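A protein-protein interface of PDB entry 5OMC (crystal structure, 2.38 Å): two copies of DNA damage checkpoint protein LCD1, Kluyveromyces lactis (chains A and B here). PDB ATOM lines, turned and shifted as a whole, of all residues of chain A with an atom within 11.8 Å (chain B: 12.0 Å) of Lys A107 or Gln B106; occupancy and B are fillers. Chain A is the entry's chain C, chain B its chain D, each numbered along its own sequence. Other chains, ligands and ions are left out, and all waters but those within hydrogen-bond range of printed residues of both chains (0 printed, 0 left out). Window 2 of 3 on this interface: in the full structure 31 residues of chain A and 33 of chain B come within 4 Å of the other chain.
Arg B99 touches Glu A98 (NH1 to CG, 3.9 Å).
CG of Glu B98 touches NH1 of Arg A99, 3.4 Å away.
Arg A99 touches Met B102.
Met A102 touches Met B102 (CE to CB, 3.6 Å).
Met A102 touches Leu B103 (CE to CD2, 3.8 Å).
Lys A107 touches Gln B106.
Of the 11 printed residues of chain A, 4 touch a printed residue of chain B.
Hydrophobic or aromatic side chains of chain A within 4 Å of the printed part of chain B: Met A102.
Hydrophobic or aromatic side chains of chain B that line the printed part of chain A: Met B102 and Leu B103.
Along chain B the printed residues that touch a printed residue of chain A span positions 98 to 106.
Among the printed residues, 6 pairs touch across the chains.
Of chain B, only Met B102 and Leu B103 come within 4 Å of Met A102.
No residue of chain B comes within 4 Å of Gln A106.
Of chain B, only Gln B106 (3.7 Å) comes within 4 Å of Lys A107.
No residue of chain B comes within 4 Å of His A108.
Of the printed residues of chain A, Glu B98 touches Arg A99.
Of the printed residues of chain A, Arg B99 touches Glu A98 (3.9 Å).
Leu B103 touches just one residue of chain A: Met A102 (3.8 Å).
Leu B104 touches none of the printed residues of chain A.
Glu B105 touches none of the printed residues of chain A.
Gln B106 touches just one residue of chain A: Lys A107.
Glu A98 touches Arg B99, and with the chains exchanged Arg A99 touches Glu B98.
Arg A99 touches Met B102, but with the chains exchanged Met A102 does not touch Arg B99 (4.3 Å).
Met A102 touches its own counterpart, Met B102.
Lys A107 touches Gln B106, but with the chains exchanged Gln A106 does not touch Lys B107 (11.0 Å).
Positions printed for both chains: 98, 99, 100, 101, 102, 103, 104, 105, 106, 107 and 108.
Of the 6 pairs that touch across the chains among the printed residues, 3 have their exchanged pair printed and touching as well.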
ATOM      1  N   GLU A  98      13.199  -6.075 -17.663  1.00  0.00           N
ATOM      2  CA  GLU A  98      14.309  -5.573 -16.869  1.00  0.00           C
ATOM      3  C   GLU A  98      14.415  -6.315 -15.557  1.00  0.00           C
ATOM      4  O   GLU A  98      15.461  -6.879 -15.263  1.00  0.00           O
ATOM      5  CB  GLU A  98      14.199  -4.053 -16.666  1.00  0.00           C
ATOM      6  CG  GLU A  98      15.545  -3.351 -16.587  1.00  0.00           C
ATOM      7  CD  GLU A  98      16.619  -3.883 -17.519  1.00  0.00           C
ATOM      8  OE1 GLU A  98      17.593  -4.499 -17.020  1.00  0.00           O
ATOM      9  OE2 GLU A  98      16.425  -3.773 -18.753  1.00  0.00           O
ATOM     10  N   ARG A  99      13.300  -6.411 -14.822  1.00  0.00           N
ATOM     11  CA  ARG A  99      13.197  -7.134 -13.560  1.00  0.00           C
ATOM     12  C   ARG A  99      13.537  -8.624 -13.747  1.00  0.00           C
ATOM     13  O   ARG A  99      14.291  -9.174 -12.940  1.00  0.00           O
ATOM     14  CB  ARG A  99      11.800  -6.930 -12.966  1.00  0.00           C
ATOM     15  CG  ARG A  99      11.487  -7.860 -11.801  1.00  0.00           C
ATOM     16  CD  ARG A  99      10.271  -7.417 -11.028  1.00  0.00           C
ATOM     17  NE  ARG A  99       9.027  -7.660 -11.757  1.00  0.00           N
ATOM     18  CZ  ARG A  99       7.829  -7.288 -11.323  1.00  0.00           C
ATOM     19  NH1 ARG A  99       7.698  -6.699 -10.146  1.00  0.00           N
ATOM     20  NH2 ARG A  99       6.748  -7.547 -12.038  1.00  0.00           N
ATOM     21  N   LYS A 100      13.054  -9.251 -14.838  1.00  0.00           N
ATOM     22  CA  LYS A 100      13.360 -10.656 -15.166  1.00  0.00           C
ATOM     23  C   LYS A 100      14.864 -10.833 -15.517  1.00  0.00           C
ATOM     24  O   LYS A 100      15.458 -11.835 -15.140  1.00  0.00           O
ATOM     25  CB  LYS A 100      12.381 -11.171 -16.240  1.00  0.00           C
ATOM     26  CG  LYS A 100      12.927 -11.944 -17.424  1.00  0.00           C
ATOM     27  CD  LYS A 100      12.017 -11.752 -18.604  1.00  0.00           C
ATOM     28  CE  LYS A 100      12.774 -11.748 -19.917  1.00  0.00           C
ATOM     29  NZ  LYS A 100      11.856 -11.626 -21.080  1.00  0.00           N
ATOM     30  N   PHE A 101      15.498  -9.813 -16.121  1.00  0.00           N
ATOM     31  CA  PHE A 101      16.932  -9.821 -16.433  1.00  0.00           C
ATOM     32  C   PHE A 101      17.726  -9.722 -15.178  1.00  0.00           C
ATOM     33  O   PHE A 101      18.768 -10.375 -15.071  1.00  0.00           O
ATOM     34  CB  PHE A 101      17.324  -8.690 -17.397  1.00  0.00           C
ATOM     35  CG  PHE A 101      16.798  -8.887 -18.790  1.00  0.00           C
ATOM     36  CD1 PHE A 101      16.512 -10.160 -19.270  1.00  0.00           C
ATOM     37  CD2 PHE A 101      16.593  -7.808 -19.628  1.00  0.00           C
ATOM     38  CE1 PHE A 101      15.973 -10.342 -20.542  1.00  0.00           C
ATOM     39  CE2 PHE A 101      16.016  -7.986 -20.882  1.00  0.00           C
ATOM     40  CZ  PHE A 101      15.724  -9.258 -21.338  1.00  0.00           C
ATOM     41  N   MET A 102      17.223  -8.934 -14.218  1.00  0.00           N
ATOM     42  CA  MET A 102      17.866  -8.732 -12.928  1.00  0.00           C
ATOM     43  C   MET A 102      17.815 -10.014 -12.111  1.00  0.00           C
ATOM     44  O   MET A 102      18.800 -10.352 -11.459  1.00  0.00           O
ATOM     45  CB  MET A 102      17.223  -7.578 -12.153  1.00  0.00           C
ATOM     46  CG  MET A 102      17.542  -6.210 -12.706  1.00  0.00           C
ATOM     47  SD  MET A 102      16.681  -4.896 -11.788  1.00  0.00           S
ATOM     48  CE  MET A 102      17.552  -4.976 -10.131  1.00  0.00           C
ATOM     49  N   LEU A 103      16.677 -10.736 -12.136  1.00  0.00           N
ATOM     50  CA  LEU A 103      16.578 -11.997 -11.402  1.00  0.00           C
ATOM     51  C   LEU A 103      17.485 -13.050 -12.039  1.00  0.00           C
ATOM     52  O   LEU A 103      18.208 -13.761 -11.336  1.00  0.00           O
ATOM     53  CB  LEU A 103      15.131 -12.487 -11.291  1.00  0.00           C
ATOM     54  CG  LEU A 103      14.185 -11.558 -10.484  1.00  0.00           C
ATOM     55  CD1 LEU A 103      12.708 -11.849 -10.773  1.00  0.00           C
ATOM     56  CD2 LEU A 103      14.469 -11.627  -9.026  1.00  0.00           C
ATOM     57  N   LEU A 104      17.521 -13.087 -13.375  1.00  0.00           N
ATOM     58  CA  LEU A 104      18.334 -14.056 -14.101  1.00  0.00           C
ATOM     59  C   LEU A 104      19.821 -13.885 -13.864  1.00  0.00           C
ATOM     60  O   LEU A 104      20.495 -14.883 -13.615  1.00  0.00           O
ATOM     61  CB  LEU A 104      17.992 -14.075 -15.590  1.00  0.00           C
ATOM     62  CG  LEU A 104      16.709 -14.853 -15.957  1.00  0.00           C
ATOM     63  CD1 LEU A 104      16.210 -14.485 -17.359  1.00  0.00           C
ATOM     64  CD2 LEU A 104      16.884 -16.351 -15.770  1.00  0.00           C
ATOM     65  N   GLU A 105      20.364 -12.668 -13.993  1.00  0.00           N
ATOM     66  CA  GLU A 105      21.797 -12.450 -13.728  1.00  0.00           C
ATOM     67  C   GLU A 105      21.916 -12.332 -12.186  1.00  0.00           C
ATOM     68  O   GLU A 105      20.950 -11.929 -11.537  1.00  0.00           O
ATOM     69  CB  GLU A 105      22.354 -11.249 -14.516  1.00  0.00           C
ATOM     70  CG  GLU A 105      21.777  -9.910 -14.117  1.00  0.00           C
ATOM     71  CD  GLU A 105      22.465  -8.639 -14.590  1.00  0.00           C
ATOM     72  OE1 GLU A 105      21.857  -7.559 -14.402  1.00  0.00           O
ATOM     73  OE2 GLU A 105      23.599  -8.705 -15.123  1.00  0.00           O
ATOM     74  N   GLN A 106      23.005 -12.785 -11.573  1.00  0.00           N
ATOM     75  CA  GLN A 106      22.985 -12.765 -10.102  1.00  0.00           C
ATOM     76  C   GLN A 106      24.000 -11.796  -9.486  1.00  0.00           C
ATOM     77  O   GLN A 106      25.145 -12.184  -9.238  1.00  0.00           O
ATOM     78  CB  GLN A 106      23.153 -14.198  -9.543  1.00  0.00           C
ATOM     79  CG  GLN A 106      22.245 -15.266 -10.175  1.00  0.00           C
ATOM     80  CD  GLN A 106      20.965 -15.548  -9.427  1.00  0.00           C
ATOM     81  OE1 GLN A 106      20.457 -16.667  -9.453  1.00  0.00           O
ATOM     82  NE2 GLN A 106      20.377 -14.545  -8.798  1.00  0.00           N
ATOM     83  N   LYS A 107      23.588 -10.544  -9.218  1.00  0.00           N
ATOM     84  CA  LYS A 107      24.527  -9.568  -8.650  1.00  0.00           C
ATOM     85  C   LYS A 107      24.741  -9.761  -7.092  1.00  0.00           C
ATOM     86  O   LYS A 107      24.136  -9.073  -6.257  1.00  0.00           O
ATOM     87  CB  LYS A 107      24.142  -8.139  -9.056  1.00  0.00           C
ATOM     88  CG  LYS A 107      24.337  -7.889 -10.561  1.00  0.00           C
ATOM     89  CD  LYS A 107      24.615  -6.415 -10.900  1.00  0.00           C
ATOM     90  CE  LYS A 107      25.164  -6.251 -12.301  1.00  0.00           C
ATOM     91  NZ  LYS A 107      25.335  -4.825 -12.688  1.00  0.00           N
ATOM     92  N   HIS A 108      25.649 -10.729  -6.750  1.00  0.00           N
ATOM     93  CA  HIS A 108      26.064 -11.180  -5.411  1.00  0.00           C
ATOM     94  C   HIS A 108      26.621 -10.049  -4.537  1.00  0.00           C
ATOM     95  O   HIS A 108      27.826  -9.785  -4.529  1.00  0.00           O
ATOM     96  CB  HIS A 108      27.084 -12.342  -5.525  1.00  0.00           C
ATOM     97  CG  HIS A 108      26.533 -13.580  -6.171  1.00  0.00           C
ATOM     98  ND1 HIS A 108      26.809 -13.889  -7.487  1.00  0.00           N
ATOM     99  CD2 HIS A 108      25.724 -14.539  -5.660  1.00  0.00           C
ATOM    100  CE1 HIS A 108      26.166 -15.021  -7.734  1.00  0.00           C
ATOM    101  NE2 HIS A 108      25.498 -15.448  -6.665  1.00  0.00           N
ATOM    102  N   ASP B  97       9.117   1.789  -9.310  1.00  0.00           N
ATOM    103  CA  ASP B  97       9.402   1.679  -7.876  1.00  0.00           C
ATOM    104  C   ASP B  97       9.983   0.329  -7.478  1.00  0.00           C
ATOM    105  O   ASP B  97      10.923   0.279  -6.677  1.00  0.00           O
ATOM    106  CB  ASP B  97       8.156   2.035  -7.052  1.00  0.00           C
ATOM    107  CG  ASP B  97       7.774   3.504  -7.175  1.00  0.00           C
ATOM    108  OD1 ASP B  97       8.650   4.312  -7.532  1.00  0.00           O
ATOM    109  OD2 ASP B  97       6.605   3.843  -6.886  1.00  0.00           O
ATOM    110  N   GLU B  98       9.465  -0.759  -8.082  1.00  0.00           N
ATOM    111  CA  GLU B  98       9.925  -2.121  -7.821  1.00  0.00           C
ATOM    112  C   GLU B  98      11.388  -2.268  -8.155  1.00  0.00           C
ATOM    113  O   GLU B  98      12.157  -2.683  -7.289  1.00  0.00           O
ATOM    114  CB  GLU B  98       9.052  -3.148  -8.567  1.00  0.00           C
ATOM    115  CG  GLU B  98       8.887  -4.456  -7.821  1.00  0.00           C
ATOM    116  CD  GLU B  98       8.779  -4.350  -6.310  1.00  0.00           C
ATOM    117  OE1 GLU B  98       9.731  -4.783  -5.620  1.00  0.00           O
ATOM    118  OE2 GLU B  98       7.781  -3.772  -5.821  1.00  0.00           O
ATOM    119  N   ARG B  99      11.786  -1.852  -9.371  1.00  0.00           N
ATOM    120  CA  ARG B  99      13.173  -1.866  -9.864  1.00  0.00           C
ATOM    121  C   ARG B  99      14.044  -1.006  -8.951  1.00  0.00           C
ATOM    122  O   ARG B  99      15.133  -1.445  -8.562  1.00  0.00           O
ATOM    123  CB  ARG B  99      13.244  -1.374 -11.323  1.00  0.00           C
ATOM    124  CG  ARG B  99      14.651  -1.107 -11.809  1.00  0.00           C
ATOM    125  CD  ARG B  99      14.756  -0.795 -13.280  1.00  0.00           C
ATOM    126  NE  ARG B  99      14.305   0.562 -13.579  1.00  0.00           N
ATOM    127  CZ  ARG B  99      14.369   1.101 -14.781  1.00  0.00           C
ATOM    128  NH1 ARG B  99      14.904   0.423 -15.791  1.00  0.00           N
ATOM    129  NH2 ARG B  99      13.898   2.320 -14.989  1.00  0.00           N
ATOM    130  N   LYS B 100      13.536   0.206  -8.579  1.00  0.00           N
ATOM    131  CA  LYS B 100      14.198   1.162  -7.678  1.00  0.00           C
ATOM    132  C   LYS B 100      14.550   0.477  -6.357  1.00  0.00           C
ATOM    133  O   LYS B 100      15.694   0.582  -5.911  1.00  0.00           O
ATOM    134  CB  LYS B 100      13.324   2.422  -7.462  1.00  0.00           C
ATOM    135  CG  LYS B 100      13.729   3.238  -6.238  1.00  0.00           C
ATOM    136  CD  LYS B 100      12.716   4.244  -5.873  1.00  0.00           C
ATOM    137  CE  LYS B 100      11.529   3.681  -5.183  1.00  0.00           C
ATOM    138  NZ  LYS B 100      10.488   4.727  -5.029  1.00  0.00           N
ATOM    139  N   PHE B 101      13.581  -0.257  -5.761  1.00  0.00           N
ATOM    140  CA  PHE B 101      13.799  -1.008  -4.526  1.00  0.00           C
ATOM    141  C   PHE B 101      14.766  -2.157  -4.691  1.00  0.00           C
ATOM    142  O   PHE B 101      15.615  -2.346  -3.825  1.00  0.00           O
ATOM    143  CB  PHE B 101      12.469  -1.469  -3.921  1.00  0.00           C
ATOM    144  CG  PHE B 101      11.684  -0.304  -3.373  1.00  0.00           C
ATOM    145  CD1 PHE B 101      12.307   0.675  -2.594  1.00  0.00           C
ATOM    146  CD2 PHE B 101      10.319  -0.195  -3.607  1.00  0.00           C
ATOM    147  CE1 PHE B 101      11.581   1.742  -2.070  1.00  0.00           C
ATOM    148  CE2 PHE B 101       9.601   0.899  -3.122  1.00  0.00           C
ATOM    149  CZ  PHE B 101      10.229   1.848  -2.332  1.00  0.00           C
ATOM    150  N   MET B 102      14.664  -2.908  -5.810  1.00  0.00           N
ATOM    151  CA  MET B 102      15.570  -4.024  -6.113  1.00  0.00           C
ATOM    152  C   MET B 102      17.007  -3.524  -6.190  1.00  0.00           C
ATOM    153  O   MET B 102      17.902  -4.193  -5.685  1.00  0.00           O
ATOM    154  CB  MET B 102      15.197  -4.708  -7.425  1.00  0.00           C
ATOM    155  CG  MET B 102      13.944  -5.541  -7.370  1.00  0.00           C
ATOM    156  SD  MET B 102      13.507  -6.252  -9.009  1.00  0.00           S
ATOM    157  CE  MET B 102      14.683  -7.621  -9.072  1.00  0.00           C
ATOM    158  N   LEU B 103      17.234  -2.337  -6.784  1.00  0.00           N
ATOM    159  CA  LEU B 103      18.585  -1.763  -6.848  1.00  0.00           C
ATOM    160  C   LEU B 103      19.042  -1.336  -5.467  1.00  0.00           C
ATOM    161  O   LEU B 103      20.176  -1.598  -5.097  1.00  0.00           O
ATOM    162  CB  LEU B 103      18.676  -0.590  -7.850  1.00  0.00           C
ATOM    163  CG  LEU B 103      18.457  -0.961  -9.313  1.00  0.00           C
ATOM    164  CD1 LEU B 103      18.221   0.255 -10.134  1.00  0.00           C
ATOM    165  CD2 LEU B 103      19.613  -1.765  -9.877  1.00  0.00           C
ATOM    166  N   LEU B 104      18.159  -0.728  -4.695  1.00  0.00           N
ATOM    167  CA  LEU B 104      18.494  -0.304  -3.345  1.00  0.00           C
ATOM    168  C   LEU B 104      18.863  -1.485  -2.453  1.00  0.00           C
ATOM    169  O   LEU B 104      19.794  -1.361  -1.680  1.00  0.00           O
ATOM    170  CB  LEU B 104      17.373   0.551  -2.732  1.00  0.00           C
ATOM    171  CG  LEU B 104      17.330   2.003  -3.192  1.00  0.00           C
ATOM    172  CD1 LEU B 104      16.036   2.667  -2.766  1.00  0.00           C
ATOM    173  CD2 LEU B 104      18.512   2.786  -2.665  1.00  0.00           C
ATOM    174  N   GLU B 105      18.217  -2.660  -2.655  1.00  0.00           N
ATOM    175  CA  GLU B 105      18.509  -3.863  -1.902  1.00  0.00           C
ATOM    176  C   GLU B 105      19.879  -4.434  -2.339  1.00  0.00           C
ATOM    177  O   GLU B 105      20.721  -4.730  -1.482  1.00  0.00           O
ATOM    178  CB  GLU B 105      17.325  -4.866  -1.948  1.00  0.00           C
ATOM    179  CG  GLU B 105      17.310  -5.906  -3.058  1.00  0.00           C
ATOM    180  CD  GLU B 105      16.169  -6.908  -3.016  1.00  0.00           C
ATOM    181  OE1 GLU B 105      15.543  -7.138  -4.079  1.00  0.00           O
ATOM    182  OE2 GLU B 105      15.919  -7.485  -1.932  1.00  0.00           O
ATOM    183  N   GLN B 106      20.144  -4.437  -3.661  1.00  0.00           N
ATOM    184  CA  GLN B 106      21.391  -4.889  -4.294  1.00  0.00           C
ATOM    185  C   GLN B 106      22.642  -4.153  -3.743  1.00  0.00           C
ATOM    186  O   GLN B 106      23.751  -4.686  -3.845  1.00  0.00           O
ATOM    187  CB  GLN B 106      21.273  -4.713  -5.813  1.00  0.00           C
ATOM    188  CG  GLN B 106      22.200  -5.580  -6.638  1.00  0.00           C
ATOM    189  CD  GLN B 106      22.201  -5.089  -8.060  1.00  0.00           C
ATOM    190  OE1 GLN B 106      22.916  -4.138  -8.416  1.00  0.00           O
ATOM    191  NE2 GLN B 106      21.362  -5.694  -8.895  1.00  0.00           N
ATOM    192  N   LYS B 107      22.463  -2.952  -3.144  1.00  0.00           N
ATOM    193  CA  LYS B 107      23.558  -2.199  -2.525  1.00  0.00           C
ATOM    194  C   LYS B 107      23.408  -2.054  -0.993  1.00  0.00           C
ATOM    195  O   LYS B 107      24.405  -2.105  -0.282  1.00  0.00           O
ATOM    196  CB  LYS B 107      23.804  -0.833  -3.205  1.00  0.00           C
ATOM    197  CG  LYS B 107      22.690   0.199  -3.057  1.00  0.00           C
ATOM    198  CD  LYS B 107      23.057   1.557  -3.670  1.00  0.00           C
ATOM    199  CE  LYS B 107      23.591   2.568  -2.692  1.00  0.00           C
ATOM    200  NZ  LYS B 107      23.186   3.944  -3.070  1.00  0.00           N
ATOM    201  N   HIS B 108      22.173  -1.889  -0.498  1.00  0.00           N
ATOM    202  CA  HIS B 108      21.848  -1.642   0.920  1.00  0.00           C
ATOM    203  C   HIS B 108      21.781  -2.910   1.750  1.00  0.00           C
ATOM    204  O   HIS B 108      21.710  -2.818   2.974  1.00  0.00           O
ATOM    205  CB  HIS B 108      20.534  -0.823   1.052  1.00  0.00           C
ATOM    206  CG  HIS B 108      20.702   0.671   0.926  1.00  0.00           C
ATOM    207  ND1 HIS B 108      21.490   1.243  -0.072  1.00  0.00           N
ATOM    208  CD2 HIS B 108      20.161   1.663   1.672  1.00  0.00           C
ATOM    209  CE1 HIS B 108      21.405   2.550   0.113  1.00  0.00           C
ATOM    210  NE2 HIS B 108      20.617   2.851   1.146  1.00  0.00           N
